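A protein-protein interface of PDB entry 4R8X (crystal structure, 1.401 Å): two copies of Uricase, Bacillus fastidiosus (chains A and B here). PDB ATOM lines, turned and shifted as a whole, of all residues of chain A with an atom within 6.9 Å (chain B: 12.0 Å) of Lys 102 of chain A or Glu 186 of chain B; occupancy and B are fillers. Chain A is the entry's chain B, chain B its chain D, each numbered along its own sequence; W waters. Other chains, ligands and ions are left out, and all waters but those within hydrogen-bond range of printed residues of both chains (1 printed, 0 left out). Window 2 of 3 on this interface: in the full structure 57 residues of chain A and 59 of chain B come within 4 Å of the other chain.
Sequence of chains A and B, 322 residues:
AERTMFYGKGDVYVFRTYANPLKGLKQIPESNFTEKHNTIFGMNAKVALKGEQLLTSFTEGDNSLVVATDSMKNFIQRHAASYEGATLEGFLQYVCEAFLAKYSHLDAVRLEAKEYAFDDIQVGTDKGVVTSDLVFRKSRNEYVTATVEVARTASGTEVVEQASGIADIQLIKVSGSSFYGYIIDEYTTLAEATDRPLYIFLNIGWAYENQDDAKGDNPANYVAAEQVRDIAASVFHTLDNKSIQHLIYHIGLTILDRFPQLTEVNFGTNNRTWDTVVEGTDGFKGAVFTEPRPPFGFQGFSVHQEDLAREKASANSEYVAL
No position is printed for both chains. Of the 10 pairs that touch across the chains among the printed residues, none has its exchanged pair printed and touching as well.
Printed residues of chain A that touch a printed residue of chain B: Asn 74, Phe 75, Arg 78, Lys 102, Tyr 103 and His 105. Among the printed residues, Asp or Glu carboxylates within 4 Å of a Lys or Arg side-chain nitrogen of the other chain: Lys 102 of chain A with Glu 186 of chain B.
OG1 of Thr 189 of chain B sits at hydrogen-bond distance from ND2 of Asn 74 of chain A, at 3.0 Å. ND2 of Asn 74 of chain A is in hydrogen-bond range of O of Tyr 187 of chain B (2.8 Å). The guanidinium group of Arg 78 of chain A is in hydrogen-bond range of the backbone carbonyl oxygen of Glu 186 of chain B (2.7 Å). NZ of Lys 102 of chain A lies within salt-bridge range of OE2 of Glu 186 of chain B (2.6 Å). The side-chain hydroxyl of Tyr 103 of chain A lies within hydrogen-bond range of the side-chain carboxylate of Asp 185 of chain B (2.7 Å).
Printed residues of chain A within 4 Å of Glu 186 of chain B: Arg 78 and Lys 102. No residue of chain B comes within 4 Å of Ala 98 of chain A. No residue of chain B comes within 4 Å of Ala 101 of chain A. Of chain B, only Asp 185 (2.7 Å) and Tyr 187 (3.8 Å) come within 4 Å of Tyr 103 of chain A. No residue of chain B comes within 4 Å of Ser 104 of chain A. Of the printed residues of chain A, Tyr 187 of chain B touches Asn 74, Phe 75, Arg 78 and Tyr 103. Of the printed residues of chain B, Phe 75 of chain A touches Tyr 187. Of the printed residues of chain B, Asn 74 of chain A touches Tyr 187 (2.8 Å) and Thr 189 (3.0 Å). Of the printed residues of chain A, Ile 183 of chain B touches His 105. The nearest printed residue of chain B that does not touch Lys 102 of chain A is Tyr 187 of chain B (4.3 Å). The nearest printed residue of chain A that does not touch Glu 186 of chain B is Asn 74 of chain A (6.2 Å).
The backbone NH (N) of Tyr 187 of chain B is in hydrogen-bond range of the side-chain carboxylate (OD1) of Asp 185 of chain B (2.9 Å). N of Asp 185 of chain B lies within hydrogen-bond range of OG1 of Thr 188 of chain B, at 3.1 Å. The backbone carbonyl oxygen (O) of Tyr 103 of chain A lies within hydrogen-bond range of the guanidinium group (NH2) of Arg 152 of chain A (3.0 Å).
CD2 of Phe 75 of chain A touches CE2 of Tyr 187 of chain B (3.4 Å). Arg 78 of chain A touches Tyr 187 of chain B. CE of Lys 102 of chain A touches OD2 of Asp 185 of chain B (3.6 Å). Tyr 187 of chain B touches Tyr 103 of chain A. Ile 183 of chain B touches His 105 of chain A (CD1 to CE1, 3.5 Å).
Water W1 lies within hydrogen-bond range of the side-chain hydroxyl (OH) of Tyr 103 of chain A (2.7 Å) and the side-chain carboxylate (OD1) of Asp 185 of chain B (2.7 Å).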
ATOM      1  N   ASN A  74      -2.641 -24.425 -15.188  1.00  0.00           N
ATOM      2  CA  ASN A  74      -3.359 -25.200 -16.188  1.00  0.00           C
ATOM      3  C   ASN A  74      -3.866 -24.308 -17.317  1.00  0.00           C
ATOM      4  O   ASN A  74      -3.795 -24.674 -18.487  1.00  0.00           O
ATOM      5  CB  ASN A  74      -4.543 -25.948 -15.573  1.00  0.00           C
ATOM      6  CG  ASN A  74      -4.123 -27.016 -14.597  1.00  0.00           C
ATOM      7  OD1 ASN A  74      -3.013 -27.542 -14.661  1.00  0.00           O
ATOM      8  ND2 ASN A  74      -5.025 -27.361 -13.692  1.00  0.00           N
ATOM      9  N   PHE A  75      -4.374 -23.137 -16.946  1.00  0.00           N
ATOM     10  CA  PHE A  75      -4.931 -22.200 -17.900  1.00  0.00           C
ATOM     11  C   PHE A  75      -3.861 -21.786 -18.916  1.00  0.00           C
ATOM     12  O   PHE A  75      -4.091 -21.808 -20.126  1.00  0.00           O
ATOM     13  CB  PHE A  75      -5.449 -20.992 -17.123  1.00  0.00           C
ATOM     14  CG  PHE A  75      -6.272 -20.023 -17.933  1.00  0.00           C
ATOM     15  CD1 PHE A  75      -5.674 -19.042 -18.712  1.00  0.00           C
ATOM     16  CD2 PHE A  75      -7.653 -20.059 -17.868  1.00  0.00           C
ATOM     17  CE1 PHE A  75      -6.447 -18.134 -19.433  1.00  0.00           C
ATOM     18  CE2 PHE A  75      -8.423 -19.156 -18.585  1.00  0.00           C
ATOM     19  CZ  PHE A  75      -7.813 -18.193 -19.365  1.00  0.00           C
ATOM     20  N   ARG A  78      -2.773 -24.854 -21.231  1.00  0.00           N
ATOM     21  CA  ARG A  78      -3.784 -25.161 -22.234  1.00  0.00           C
ATOM     22  C   ARG A  78      -3.855 -24.107 -23.333  1.00  0.00           C
ATOM     23  O   ARG A  78      -4.027 -24.432 -24.507  1.00  0.00           O
ATOM     24  CB  ARG A  78      -5.139 -25.393 -21.576  1.00  0.00           C
ATOM     25  CG  ARG A  78      -5.121 -26.615 -20.678  1.00  0.00           C
ATOM     26  CD  ARG A  78      -6.415 -26.820 -19.933  1.00  0.00           C
ATOM     27  NE  ARG A  78      -6.207 -27.686 -18.779  1.00  0.00           N
ATOM     28  CZ  ARG A  78      -7.166 -28.040 -17.933  1.00  0.00           C
ATOM     29  NH1 ARG A  78      -8.403 -27.602 -18.118  1.00  0.00           N
ATOM     30  NH2 ARG A  78      -6.887 -28.828 -16.906  1.00  0.00           N
ATOM     31  N   GLU A  97      -5.744 -11.651 -21.966  1.00  0.00           N
ATOM     32  CA  GLU A  97      -7.112 -11.379 -22.385  1.00  0.00           C
ATOM     33  C   GLU A  97      -8.018 -12.549 -22.068  1.00  0.00           C
ATOM     34  O   GLU A  97      -9.157 -12.358 -21.640  1.00  0.00           O
ATOM     35  CB  GLU A  97      -7.172 -10.999 -23.863  1.00  0.00           C
ATOM     36  CG  GLU A  97      -6.576  -9.618 -24.105  1.00  0.00           C
ATOM     37  CD  GLU A  97      -6.379  -9.296 -25.570  1.00  0.00           C
ATOM     38  OE1 GLU A  97      -5.939  -8.171 -25.872  1.00  0.00           O
ATOM     39  OE2 GLU A  97      -6.650 -10.165 -26.415  1.00  0.00           O
ATOM     40  N   ALA A  98      -7.508 -13.766 -22.235  1.00  0.00           N
ATOM     41  CA  ALA A  98      -8.316 -14.941 -21.927  1.00  0.00           C
ATOM     42  C   ALA A  98      -8.666 -15.044 -20.440  1.00  0.00           C
ATOM     43  O   ALA A  98      -9.789 -15.411 -20.090  1.00  0.00           O
ATOM     44  CB  ALA A  98      -7.648 -16.216 -22.429  1.00  0.00           C
ATOM     45  N   PHE A  99      -7.712 -14.725 -19.567  1.00  0.00           N
ATOM     46  CA  PHE A  99      -7.982 -14.702 -18.139  1.00  0.00           C
ATOM     47  C   PHE A  99      -9.096 -13.705 -17.828  1.00  0.00           C
ATOM     48  O   PHE A  99     -10.008 -14.008 -17.061  1.00  0.00           O
ATOM     49  CB  PHE A  99      -6.724 -14.308 -17.350  1.00  0.00           C
ATOM     50  CG  PHE A  99      -5.856 -15.469 -16.929  1.00  0.00           C
ATOM     51  CD1 PHE A  99      -6.328 -16.440 -16.043  1.00  0.00           C
ATOM     52  CD2 PHE A  99      -4.553 -15.547 -17.373  1.00  0.00           C
ATOM     53  CE1 PHE A  99      -5.522 -17.501 -15.637  1.00  0.00           C
ATOM     54  CE2 PHE A  99      -3.716 -16.598 -16.957  1.00  0.00           C
ATOM     55  CZ  PHE A  99      -4.210 -17.579 -16.087  1.00  0.00           C
ATOM     56  N   LEU A 100      -9.014 -12.506 -18.404  1.00  0.00           N
ATOM     57  CA  LEU A 100     -10.030 -11.486 -18.134  1.00  0.00           C
ATOM     58  C   LEU A 100     -11.409 -11.858 -18.691  1.00  0.00           C
ATOM     59  O   LEU A 100     -12.430 -11.507 -18.103  1.00  0.00           O
ATOM     60  CB  LEU A 100      -9.584 -10.116 -18.648  1.00  0.00           C
ATOM     61  CG  LEU A 100      -8.418  -9.490 -17.879  1.00  0.00           C
ATOM     62  CD1 LEU A 100      -7.894  -8.284 -18.644  1.00  0.00           C
ATOM     63  CD2 LEU A 100      -8.842  -9.082 -16.470  1.00  0.00           C
ATOM     64  N   ALA A 101     -11.441 -12.570 -19.813  1.00  0.00           N
ATOM     65  CA  ALA A 101     -12.709 -13.018 -20.389  1.00  0.00           C
ATOM     66  C   ALA A 101     -13.353 -14.082 -19.511  1.00  0.00           C
ATOM     67  O   ALA A 101     -14.569 -14.180 -19.435  1.00  0.00           O
ATOM     68  CB  ALA A 101     -12.498 -13.549 -21.792  1.00  0.00           C
ATOM     69  N   LYS A 102     -12.532 -14.884 -18.849  1.00  0.00           N
ATOM     70  CA  LYS A 102     -13.035 -15.985 -18.038  1.00  0.00           C
ATOM     71  C   LYS A 102     -13.458 -15.526 -16.641  1.00  0.00           C
ATOM     72  O   LYS A 102     -14.428 -16.035 -16.074  1.00  0.00           O
ATOM     73  CB  LYS A 102     -11.961 -17.070 -17.931  1.00  0.00           C
ATOM     74  CG  LYS A 102     -12.365 -18.277 -17.104  1.00  0.00           C
ATOM     75  CD  LYS A 102     -13.498 -19.055 -17.736  1.00  0.00           C
ATOM     76  CE  LYS A 102     -13.911 -20.203 -16.841  1.00  0.00           C
ATOM     77  NZ  LYS A 102     -15.035 -20.995 -17.425  1.00  0.00           N
ATOM     78  N   TYR A 103     -12.710 -14.580 -16.078  1.00  0.00           N
ATOM     79  CA  TYR A 103     -12.890 -14.203 -14.678  1.00  0.00           C
ATOM     80  C   TYR A 103     -13.267 -12.733 -14.545  1.00  0.00           C
ATOM     81  O   TYR A 103     -12.409 -11.854 -14.533  1.00  0.00           O
ATOM     82  CB  TYR A 103     -11.628 -14.550 -13.874  1.00  0.00           C
ATOM     83  CG  TYR A 103     -11.306 -16.025 -13.941  1.00  0.00           C
ATOM     84  CD1 TYR A 103     -12.157 -16.958 -13.365  1.00  0.00           C
ATOM     85  CD2 TYR A 103     -10.179 -16.490 -14.616  1.00  0.00           C
ATOM     86  CE1 TYR A 103     -11.881 -18.313 -13.430  1.00  0.00           C
ATOM     87  CE2 TYR A 103      -9.896 -17.841 -14.687  1.00  0.00           C
ATOM     88  CZ  TYR A 103     -10.756 -18.749 -14.095  1.00  0.00           C
ATOM     89  OH  TYR A 103     -10.492 -20.100 -14.163  1.00  0.00           O
ATOM     90  N   SER A 104     -14.572 -12.476 -14.451  1.00  0.00           N
ATOM     91  CA  SER A 104     -15.082 -11.109 -14.463  1.00  0.00           C
ATOM     92  C   SER A 104     -14.656 -10.302 -13.237  1.00  0.00           C
ATOM     93  O   SER A 104     -14.608  -9.074 -13.289  1.00  0.00           O
ATOM     94  CB  SER A 104     -16.607 -11.113 -14.586  1.00  0.00           C
ATOM     95  OG  SER A 104     -17.199 -11.744 -13.466  1.00  0.00           O
ATOM     96  N   HIS A 105     -14.339 -10.989 -12.144  1.00  0.00           N
ATOM     97  CA  HIS A 105     -13.970 -10.321 -10.891  1.00  0.00           C
ATOM     98  C   HIS A 105     -12.530  -9.797 -10.889  1.00  0.00           C
ATOM     99  O   HIS A 105     -12.129  -9.067  -9.984  1.00  0.00           O
ATOM    100  CB  HIS A 105     -14.201 -11.249  -9.688  1.00  0.00           C
ATOM    101  CG  HIS A 105     -13.346 -12.476  -9.704  1.00  0.00           C
ATOM    102  ND1 HIS A 105     -13.631 -13.570 -10.493  1.00  0.00           N
ATOM    103  CD2 HIS A 105     -12.207 -12.782  -9.037  1.00  0.00           C
ATOM    104  CE1 HIS A 105     -12.707 -14.495 -10.312  1.00  0.00           C
ATOM    105  NE2 HIS A 105     -11.825 -14.039  -9.439  1.00  0.00           N
ATOM    106  N   LEU A 106     -11.749 -10.175 -11.894  1.00  0.00           N
ATOM    107  CA  LEU A 106     -10.392  -9.663 -12.018  1.00  0.00           C
ATOM    108  C   LEU A 106     -10.416  -8.382 -12.813  1.00  0.00           C
ATOM    109  O   LEU A 106     -11.244  -8.222 -13.710  1.00  0.00           O
ATOM    110  CB  LEU A 106      -9.515 -10.652 -12.768  1.00  0.00           C
ATOM    111  CG  LEU A 106      -9.338 -12.039 -12.175  1.00  0.00           C
ATOM    112  CD1 LEU A 106      -8.462 -12.860 -13.104  1.00  0.00           C
ATOM    113  CD2 LEU A 106      -8.724 -11.919 -10.795  1.00  0.00           C
ATOM    114  N   ARG A 152      -8.759  -3.844 -17.510  1.00  0.00           N
ATOM    115  CA  ARG A 152     -10.049  -3.412 -18.038  1.00  0.00           C
ATOM    116  C   ARG A 152     -10.066  -1.916 -18.297  1.00  0.00           C
ATOM    117  O   ARG A 152      -9.338  -1.144 -17.656  1.00  0.00           O
ATOM    118  CB  ARG A 152     -11.208  -3.801 -17.110  1.00  0.00           C
ATOM    119  CG  ARG A 152     -11.284  -5.313 -16.879  1.00  0.00           C
ATOM    120  CD  ARG A 152     -12.611  -5.752 -16.259  1.00  0.00           C
ATOM    121  NE  ARG A 152     -12.533  -7.154 -15.856  1.00  0.00           N
ATOM    122  CZ  ARG A 152     -12.675  -8.179 -16.691  1.00  0.00           C
ATOM    123  NH1 ARG A 152     -12.933  -7.957 -17.975  1.00  0.00           N
ATOM    124  NH2 ARG A 152     -12.566  -9.425 -16.244  1.00  0.00           N
ATOM    125  N   TYR B 182     -11.845 -22.475  -3.061  1.00  0.00           N
ATOM    126  CA  TYR B 182     -11.456 -21.844  -4.324  1.00  0.00           C
ATOM    127  C   TYR B 182     -12.514 -21.960  -5.404  1.00  0.00           C
ATOM    128  O   TYR B 182     -13.410 -22.800  -5.336  1.00  0.00           O
ATOM    129  CB  TYR B 182     -10.195 -22.502  -4.882  1.00  0.00           C
ATOM    130  CG  TYR B 182      -9.011 -22.483  -3.966  1.00  0.00           C
ATOM    131  CD1 TYR B 182      -8.196 -21.365  -3.885  1.00  0.00           C
ATOM    132  CD2 TYR B 182      -8.684 -23.596  -3.202  1.00  0.00           C
ATOM    133  CE1 TYR B 182      -7.096 -21.345  -3.054  1.00  0.00           C
ATOM    134  CE2 TYR B 182      -7.586 -23.587  -2.372  1.00  0.00           C
ATOM    135  CZ  TYR B 182      -6.797 -22.458  -2.302  1.00  0.00           C
ATOM    136  OH  TYR B 182      -5.704 -22.441  -1.479  1.00  0.00           O
ATOM    137  N   ILE B 183     -12.369 -21.128  -6.428  1.00  0.00           N
ATOM    138  CA  ILE B 183     -13.148 -21.270  -7.644  1.00  0.00           C
ATOM    139  C   ILE B 183     -12.820 -22.620  -8.268  1.00  0.00           C
ATOM    140  O   ILE B 183     -11.655 -23.012  -8.358  1.00  0.00           O
ATOM    141  CB  ILE B 183     -12.831 -20.136  -8.629  1.00  0.00           C
ATOM    142  CG1 ILE B 183     -13.478 -18.836  -8.153  1.00  0.00           C
ATOM    143  CG2 ILE B 183     -13.290 -20.484 -10.039  1.00  0.00           C
ATOM    144  CD1 ILE B 183     -12.932 -17.605  -8.826  1.00  0.00           C
ATOM    145  N   ILE B 184     -13.855 -23.345  -8.673  1.00  0.00           N
ATOM    146  CA  ILE B 184     -13.679 -24.647  -9.290  1.00  0.00           C
ATOM    147  C   ILE B 184     -14.321 -24.603 -10.662  1.00  0.00           C
ATOM    148  O   ILE B 184     -15.511 -24.329 -10.784  1.00  0.00           O
ATOM    149  CB  ILE B 184     -14.324 -25.747  -8.435  1.00  0.00           C
ATOM    150  CG1 ILE B 184     -13.700 -25.753  -7.033  1.00  0.00           C
ATOM    151  CG2 ILE B 184     -14.198 -27.109  -9.117  1.00  0.00           C
ATOM    152  CD1 ILE B 184     -14.228 -26.839  -6.120  1.00  0.00           C
ATOM    153  N   ASP B 185     -13.525 -24.829 -11.698  1.00  0.00           N
ATOM    154  CA  ASP B 185     -14.044 -24.819 -13.056  1.00  0.00           C
ATOM    155  C   ASP B 185     -13.257 -25.777 -13.930  1.00  0.00           C
ATOM    156  O   ASP B 185     -12.587 -26.670 -13.420  1.00  0.00           O
ATOM    157  CB  ASP B 185     -14.112 -23.405 -13.649  1.00  0.00           C
ATOM    158  CG  ASP B 185     -12.775 -22.695 -13.665  1.00  0.00           C
ATOM    159  OD1 ASP B 185     -11.727 -23.366 -13.702  1.00  0.00           O
ATOM    160  OD2 ASP B 185     -12.779 -21.447 -13.658  1.00  0.00           O
ATOM    161  N   GLU B 186     -13.324 -25.579 -15.240  1.00  0.00           N
ATOM    162  CA  GLU B 186     -12.688 -26.507 -16.165  1.00  0.00           C
ATOM    163  C   GLU B 186     -11.168 -26.497 -16.038  1.00  0.00           C
ATOM    164  O   GLU B 186     -10.501 -27.419 -16.500  1.00  0.00           O
ATOM    165  CB  GLU B 186     -13.112 -26.222 -17.611  1.00  0.00           C
ATOM    166  CG  GLU B 186     -12.690 -24.864 -18.142  1.00  0.00           C
ATOM    167  CD  GLU B 186     -13.765 -23.800 -17.981  1.00  0.00           C
ATOM    168  OE1 GLU B 186     -14.591 -23.901 -17.050  1.00  0.00           O
ATOM    169  OE2 GLU B 186     -13.780 -22.854 -18.795  1.00  0.00           O
ATOM    170  N   TYR B 187     -10.625 -25.469 -15.392  1.00  0.00           N
ATOM    171  CA  TYR B 187      -9.174 -25.372 -15.232  1.00  0.00           C
ATOM    172  C   TYR B 187      -8.662 -25.990 -13.940  1.00  0.00           C
ATOM    173  O   TYR B 187      -7.460 -26.031 -13.702  1.00  0.00           O
ATOM    174  CB  TYR B 187      -8.699 -23.923 -15.388  1.00  0.00           C
ATOM    175  CG  TYR B 187      -8.994 -23.407 -16.767  1.00  0.00           C
ATOM    176  CD1 TYR B 187      -8.205 -23.781 -17.850  1.00  0.00           C
ATOM    177  CD2 TYR B 187     -10.083 -22.579 -17.001  1.00  0.00           C
ATOM    178  CE1 TYR B 187      -8.484 -23.336 -19.121  1.00  0.00           C
ATOM    179  CE2 TYR B 187     -10.368 -22.117 -18.272  1.00  0.00           C
ATOM    180  CZ  TYR B 187      -9.571 -22.506 -19.329  1.00  0.00           C
ATOM    181  OH  TYR B 187      -9.851 -22.050 -20.597  1.00  0.00           O
ATOM    182  N   THR B 188      -9.580 -26.490 -13.122  1.00  0.00           N
ATOM    183  CA  THR B 188      -9.225 -27.179 -11.884  1.00  0.00           C
ATOM    184  C   THR B 188      -8.619 -28.556 -12.154  1.00  0.00           C
ATOM    185  O   THR B 188      -9.149 -29.334 -12.953  1.00  0.00           O
ATOM    186  CB  THR B 188     -10.461 -27.331 -10.989  1.00  0.00           C
ATOM    187  OG1 THR B 188     -10.924 -26.027 -10.623  1.00  0.00           O
ATOM    188  CG2 THR B 188     -10.143 -28.136  -9.732  1.00  0.00           C
ATOM    189  N   THR B 189      -7.509 -28.856 -11.487  1.00  0.00           N
ATOM    190  CA  THR B 189      -6.879 -30.161 -11.627  1.00  0.00           C
ATOM    191  C   THR B 189      -7.807 -31.224 -11.066  1.00  0.00           C
ATOM    192  O   THR B 189      -8.264 -31.113  -9.931  1.00  0.00           O
ATOM    193  CB  THR B 189      -5.520 -30.223 -10.901  1.00  0.00           C
ATOM    194  OG1 THR B 189      -4.593 -29.356 -11.558  1.00  0.00           O
ATOM    195  CG2 THR B 189      -4.965 -31.647 -10.914  1.00  0.00           C
ATOM    196  N   LEU B 190      -8.096 -32.237 -11.877  1.00  0.00           N
ATOM    197  CA  LEU B 190      -8.993 -33.315 -11.476  1.00  0.00           C
ATOM    198  C   LEU B 190      -8.263 -34.380 -10.663  1.00  0.00           C
ATOM    199  O   LEU B 190      -8.011 -35.487 -11.144  1.00  0.00           O
ATOM    200  CB  LEU B 190      -9.669 -33.935 -12.702  1.00  0.00           C
ATOM    201  CG  LEU B 190     -10.627 -33.004 -13.449  1.00  0.00           C
ATOM    202  CD1 LEU B 190     -10.976 -33.572 -14.813  1.00  0.00           C
ATOM    203  CD2 LEU B 190     -11.888 -32.772 -12.628  1.00  0.00           C
ATOM    204  N   ALA B 191      -7.922 -34.027  -9.429  1.00  0.00           N
ATOM    205  CA  ALA B 191      -7.275 -34.945  -8.505  1.00  0.00           C
ATOM    206  C   ALA B 191      -7.673 -34.612  -7.072  1.00  0.00           C
ATOM    207  O   ALA B 191      -7.981 -33.464  -6.759  1.00  0.00           O
ATOM    208  CB  ALA B 191      -5.762 -34.881  -8.664  1.00  0.00           C
HETATM  209  O   HOH W   1      -9.807 -21.996 -12.305  1.00  0.00           O
